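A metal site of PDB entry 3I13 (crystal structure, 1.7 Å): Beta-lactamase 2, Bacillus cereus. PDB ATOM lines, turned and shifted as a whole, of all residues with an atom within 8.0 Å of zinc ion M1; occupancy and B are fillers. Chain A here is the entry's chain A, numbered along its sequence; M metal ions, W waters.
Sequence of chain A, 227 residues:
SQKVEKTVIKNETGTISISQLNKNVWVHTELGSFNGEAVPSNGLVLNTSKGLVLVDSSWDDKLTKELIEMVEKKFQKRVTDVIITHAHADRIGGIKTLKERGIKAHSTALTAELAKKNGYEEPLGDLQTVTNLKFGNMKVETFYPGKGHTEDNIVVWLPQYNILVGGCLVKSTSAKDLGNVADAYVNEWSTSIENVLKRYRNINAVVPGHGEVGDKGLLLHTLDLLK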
ATOM      1  N   THR A  85      -0.498 -27.029  11.958  1.00  0.00           N
ATOM      2  CA  THR A  85      -1.084 -27.786  13.066  1.00  0.00           C
ATOM      3  C   THR A  85      -2.601 -28.055  12.936  1.00  0.00           C
ATOM      4  O   THR A  85      -3.116 -28.908  13.597  1.00  0.00           O
ATOM      5  CB  THR A  85      -0.721 -27.211  14.433  1.00  0.00           C
ATOM      6  OG1 THR A  85      -1.217 -25.877  14.492  1.00  0.00           O
ATOM      7  CG2 THR A  85       0.883 -27.280  14.693  1.00  0.00           C
ATOM      8  N   HIS A  86      -3.268 -27.325  12.043  1.00  0.00           N
ATOM      9  CA  HIS A  86      -4.646 -27.629  11.628  1.00  0.00           C
ATOM     10  C   HIS A  86      -4.998 -26.752  10.424  1.00  0.00           C
ATOM     11  O   HIS A  86      -4.252 -25.876  10.126  1.00  0.00           O
ATOM     12  CB  HIS A  86      -5.694 -27.633  12.745  1.00  0.00           C
ATOM     13  CG  HIS A  86      -6.046 -26.297  13.313  1.00  0.00           C
ATOM     14  ND1 HIS A  86      -5.319 -25.701  14.318  1.00  0.00           N
ATOM     15  CD2 HIS A  86      -7.099 -25.470  13.077  1.00  0.00           C
ATOM     16  CE1 HIS A  86      -5.872 -24.559  14.643  1.00  0.00           C
ATOM     17  NE2 HIS A  86      -6.920 -24.371  13.876  1.00  0.00           N
ATOM     18  N   ALA A  87      -6.151 -27.014   9.794  1.00  0.00           N
ATOM     19  CA  ALA A  87      -6.530 -26.448   8.516  1.00  0.00           C
ATOM     20  C   ALA A  87      -7.322 -25.133   8.600  1.00  0.00           C
ATOM     21  O   ALA A  87      -7.860 -24.684   7.592  1.00  0.00           O
ATOM     22  CB  ALA A  87      -7.378 -27.547   7.730  1.00  0.00           C
ATOM     23  N   HIS A  88      -7.376 -24.455   9.723  1.00  0.00           N
ATOM     24  CA  HIS A  88      -8.005 -23.119   9.803  1.00  0.00           C
ATOM     25  C   HIS A  88      -7.050 -21.991   9.286  1.00  0.00           C
ATOM     26  O   HIS A  88      -5.852 -22.125   9.288  1.00  0.00           O
ATOM     27  CB  HIS A  88      -8.363 -22.802  11.256  1.00  0.00           C
ATOM     28  CG  HIS A  88      -9.660 -23.396  11.752  1.00  0.00           C
ATOM     29  ND1 HIS A  88      -9.964 -23.507  13.115  1.00  0.00           N
ATOM     30  CD2 HIS A  88     -10.745 -23.860  11.092  1.00  0.00           C
ATOM     31  CE1 HIS A  88     -11.170 -24.025  13.237  1.00  0.00           C
ATOM     32  NE2 HIS A  88     -11.676 -24.223  12.033  1.00  0.00           N
ATOM     33  N   ALA A  89      -7.606 -20.816   8.938  1.00  0.00           N
ATOM     34  CA  ALA A  89      -6.827 -19.657   8.358  1.00  0.00           C
ATOM     35  C   ALA A  89      -5.647 -19.162   9.154  1.00  0.00           C
ATOM     36  O   ALA A  89      -4.570 -18.923   8.603  1.00  0.00           O
ATOM     37  CB  ALA A  89      -7.838 -18.465   8.057  1.00  0.00           C
ATOM     38  N   ASP A  90      -5.772 -19.060  10.477  1.00  0.00           N
ATOM     39  CA  ASP A  90      -4.621 -18.682  11.299  1.00  0.00           C
ATOM     40  C   ASP A  90      -3.473 -19.604  11.150  1.00  0.00           C
ATOM     41  O   ASP A  90      -2.375 -19.242  11.509  1.00  0.00           O
ATOM     42  CB  ASP A  90      -4.938 -18.520  12.828  1.00  0.00           C
ATOM     43  CG  ASP A  90      -5.697 -19.688  13.419  1.00  0.00           C
ATOM     44  OD1 ASP A  90      -6.633 -20.195  12.765  1.00  0.00           O
ATOM     45  OD2 ASP A  90      -5.428 -20.036  14.604  1.00  0.00           O
ATOM     46  N   ARG A  91      -3.711 -20.838  10.680  1.00  0.00           N
ATOM     47  CA  ARG A  91      -2.594 -21.792  10.596  1.00  0.00           C
ATOM     48  C   ARG A  91      -2.170 -21.970   9.146  1.00  0.00           C
ATOM     49  O   ARG A  91      -1.002 -22.110   8.878  1.00  0.00           O
ATOM     50  CB  ARG A  91      -2.987 -23.162  11.208  1.00  0.00           C
ATOM     51  CG  ARG A  91      -3.564 -23.017  12.644  1.00  0.00           C
ATOM     52  CD  ARG A  91      -2.511 -22.155  13.415  1.00  0.00           C
ATOM     53  NE  ARG A  91      -2.841 -21.723  14.743  1.00  0.00           N
ATOM     54  CZ  ARG A  91      -2.010 -21.016  15.512  1.00  0.00           C
ATOM     55  NH1 ARG A  91      -2.384 -20.665  16.718  1.00  0.00           N
ATOM     56  NH2 ARG A  91      -0.828 -20.599  15.084  1.00  0.00           N
ATOM     57  N   HIS A 149     -10.294 -28.841  19.384  1.00  0.00           N
ATOM     58  CA  HIS A 149     -10.574 -27.551  18.768  1.00  0.00           C
ATOM     59  C   HIS A 149     -11.062 -27.724  17.304  1.00  0.00           C
ATOM     60  O   HIS A 149     -11.962 -26.981  16.791  1.00  0.00           O
ATOM     61  CB  HIS A 149      -9.295 -26.657  18.795  1.00  0.00           C
ATOM     62  CG  HIS A 149      -9.387 -25.456  17.898  1.00  0.00           C
ATOM     63  ND1 HIS A 149     -10.159 -24.372  18.220  1.00  0.00           N
ATOM     64  CD2 HIS A 149      -8.801 -25.154  16.710  1.00  0.00           C
ATOM     65  CE1 HIS A 149     -10.117 -23.489  17.235  1.00  0.00           C
ATOM     66  NE2 HIS A 149      -9.291 -23.931  16.318  1.00  0.00           N
ATOM     67  N   THR A 150     -10.398 -28.660  16.598  1.00  0.00           N
ATOM     68  CA  THR A 150     -10.831 -29.110  15.285  1.00  0.00           C
ATOM     69  C   THR A 150     -10.629 -30.617  15.223  1.00  0.00           C
ATOM     70  O   THR A 150      -9.998 -31.229  16.101  1.00  0.00           O
ATOM     71  CB  THR A 150     -10.032 -28.493  14.117  1.00  0.00           C
ATOM     72  OG1 THR A 150      -8.635 -28.780  14.279  1.00  0.00           O
ATOM     73  CG2 THR A 150     -10.347 -26.977  14.016  1.00  0.00           C
ATOM     74  N   ASP A 152      -8.762 -32.186  13.233  1.00  0.00           N
ATOM     75  CA  ASP A 152      -7.430 -32.491  12.712  1.00  0.00           C
ATOM     76  C   ASP A 152      -6.257 -31.999  13.545  1.00  0.00           C
ATOM     77  O   ASP A 152      -5.144 -32.379  13.307  1.00  0.00           O
ATOM     78  CB  ASP A 152      -7.249 -32.045  11.271  1.00  0.00           C
ATOM     79  CG  ASP A 152      -7.384 -30.521  11.102  1.00  0.00           C
ATOM     80  OD1 ASP A 152      -8.264 -29.953  11.781  1.00  0.00           O
ATOM     81  OD2 ASP A 152      -6.624 -29.915  10.335  1.00  0.00           O
ATOM     82  N   ASN A 153      -6.550 -31.227  14.609  1.00  0.00           N
ATOM     83  CA  ASN A 153      -5.502 -30.566  15.373  1.00  0.00           C
ATOM     84  C   ASN A 153      -4.364 -31.514  15.873  1.00  0.00           C
ATOM     85  O   ASN A 153      -4.590 -32.594  16.445  1.00  0.00           O
ATOM     86  CB  ASN A 153      -6.088 -29.717  16.519  1.00  0.00           C
ATOM     87  CG  ASN A 153      -7.047 -30.447  17.499  1.00  0.00           C
ATOM     88  OD1 ASN A 153      -7.839 -29.719  18.145  1.00  0.00           O
ATOM     89  ND2 ASN A 153      -6.979 -31.766  17.674  1.00  0.00           N
ATOM     90  N   GLY A 167      -0.923 -25.497  20.163  1.00  0.00           N
ATOM     91  CA  GLY A 167      -1.855 -24.983  19.170  1.00  0.00           C
ATOM     92  C   GLY A 167      -3.211 -24.570  19.757  1.00  0.00           C
ATOM     93  O   GLY A 167      -3.345 -24.305  20.973  1.00  0.00           O
ATOM     94  N   CYS A 168      -4.246 -24.522  18.919  1.00  0.00           N
ATOM     95  CA  CYS A 168      -5.550 -24.131  19.462  1.00  0.00           C
ATOM     96  C   CYS A 168      -6.249 -25.219  20.275  1.00  0.00           C
ATOM     97  O   CYS A 168      -7.271 -24.972  20.903  1.00  0.00           O
ATOM     98  CB  CYS A 168      -6.444 -23.537  18.392  1.00  0.00           C
ATOM     99  SG  CYS A 168      -5.681 -22.031  17.722  1.00  0.00           S
ATOM    100  N   LEU A 169      -5.652 -26.410  20.344  1.00  0.00           N
ATOM    101  CA  LEU A 169      -6.144 -27.395  21.307  1.00  0.00           C
ATOM    102  C   LEU A 169      -5.957 -26.910  22.712  1.00  0.00           C
ATOM    103  O   LEU A 169      -6.626 -27.357  23.602  1.00  0.00           O
ATOM    104  CB  LEU A 169      -5.363 -28.719  21.151  1.00  0.00           C
ATOM    105  CG  LEU A 169      -5.737 -29.973  21.951  1.00  0.00           C
ATOM    106  CD1 LEU A 169      -7.015 -30.599  21.355  1.00  0.00           C
ATOM    107  CD2 LEU A 169      -4.619 -31.020  21.943  1.00  0.00           C
ATOM    108  N   ASN A 180     -13.872 -20.225  19.287  1.00  0.00           N
ATOM    109  CA  ASN A 180     -14.642 -20.740  18.174  1.00  0.00           C
ATOM    110  C   ASN A 180     -14.842 -22.258  18.231  1.00  0.00           C
ATOM    111  O   ASN A 180     -13.890 -23.019  17.941  1.00  0.00           O
ATOM    112  CB  ASN A 180     -13.905 -20.376  16.877  1.00  0.00           C
ATOM    113  CG  ASN A 180     -14.607 -20.902  15.623  1.00  0.00           C
ATOM    114  OD1 ASN A 180     -15.835 -21.160  15.629  1.00  0.00           O
ATOM    115  ND2 ASN A 180     -13.806 -21.068  14.538  1.00  0.00           N
ATOM    116  N   ASP A 183     -16.210 -25.704  14.628  1.00  0.00           N
ATOM    117  CA  ASP A 183     -15.493 -26.899  14.089  1.00  0.00           C
ATOM    118  C   ASP A 183     -14.926 -27.880  15.125  1.00  0.00           C
ATOM    119  O   ASP A 183     -14.210 -28.792  14.800  1.00  0.00           O
ATOM    120  CB  ASP A 183     -14.407 -26.445  13.147  1.00  0.00           C
ATOM    121  CG  ASP A 183     -14.949 -25.696  11.934  1.00  0.00           C
ATOM    122  OD1 ASP A 183     -16.035 -25.986  11.417  1.00  0.00           O
ATOM    123  OD2 ASP A 183     -14.186 -24.850  11.491  1.00  0.00           O
ATOM    124  N   HIS A 210      -2.943 -19.228  21.054  1.00  0.00           N
ATOM    125  CA  HIS A 210      -3.111 -17.806  21.228  1.00  0.00           C
ATOM    126  C   HIS A 210      -2.827 -17.510  22.726  1.00  0.00           C
ATOM    127  O   HIS A 210      -3.302 -18.252  23.562  1.00  0.00           O
ATOM    128  CB  HIS A 210      -4.575 -17.442  20.919  1.00  0.00           C
ATOM    129  CG  HIS A 210      -5.059 -17.859  19.544  1.00  0.00           C
ATOM    130  ND1 HIS A 210      -4.939 -17.048  18.435  1.00  0.00           N
ATOM    131  CD2 HIS A 210      -5.698 -18.982  19.125  1.00  0.00           C
ATOM    132  CE1 HIS A 210      -5.448 -17.658  17.377  1.00  0.00           C
ATOM    133  NE2 HIS A 210      -5.923 -18.829  17.765  1.00  0.00           N
HETATM  134 ZN    ZN M   1      -8.588 -23.229  14.535  1.00  0.00          ZN
HETATM  135 ZN    ZN M   2      -6.563 -20.912  16.541  1.00  0.00          ZN
HETATM  136  O   HOH W   1      -7.731 -21.304  14.737  1.00  0.00           O
HETATM  137  O   HOH W   2     -10.580 -21.337  15.171  1.00  0.00           O
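The backbone NH (N) of His 149 is in hydrogen-bond range of the side-chain amide oxygen (OD1) of Asn 153 (2.9 Å). NE2 of His 88 sits at hydrogen-bond distance from OD2 of Asp 183 (2.6 Å).
The nearest printed residue that does not touch zinc ion M1 is Asp 90 (4.02 Å).
Zinc ion M1 is bound by ND1 of His 88 (2.0 Å), NE2 of His 149 (2.0 Å), water W1 (2.1 Å) and NE2 of His 86 (2.1 Å). Slightly farther from zinc ion M1 lies water W2 (2.8 Å).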
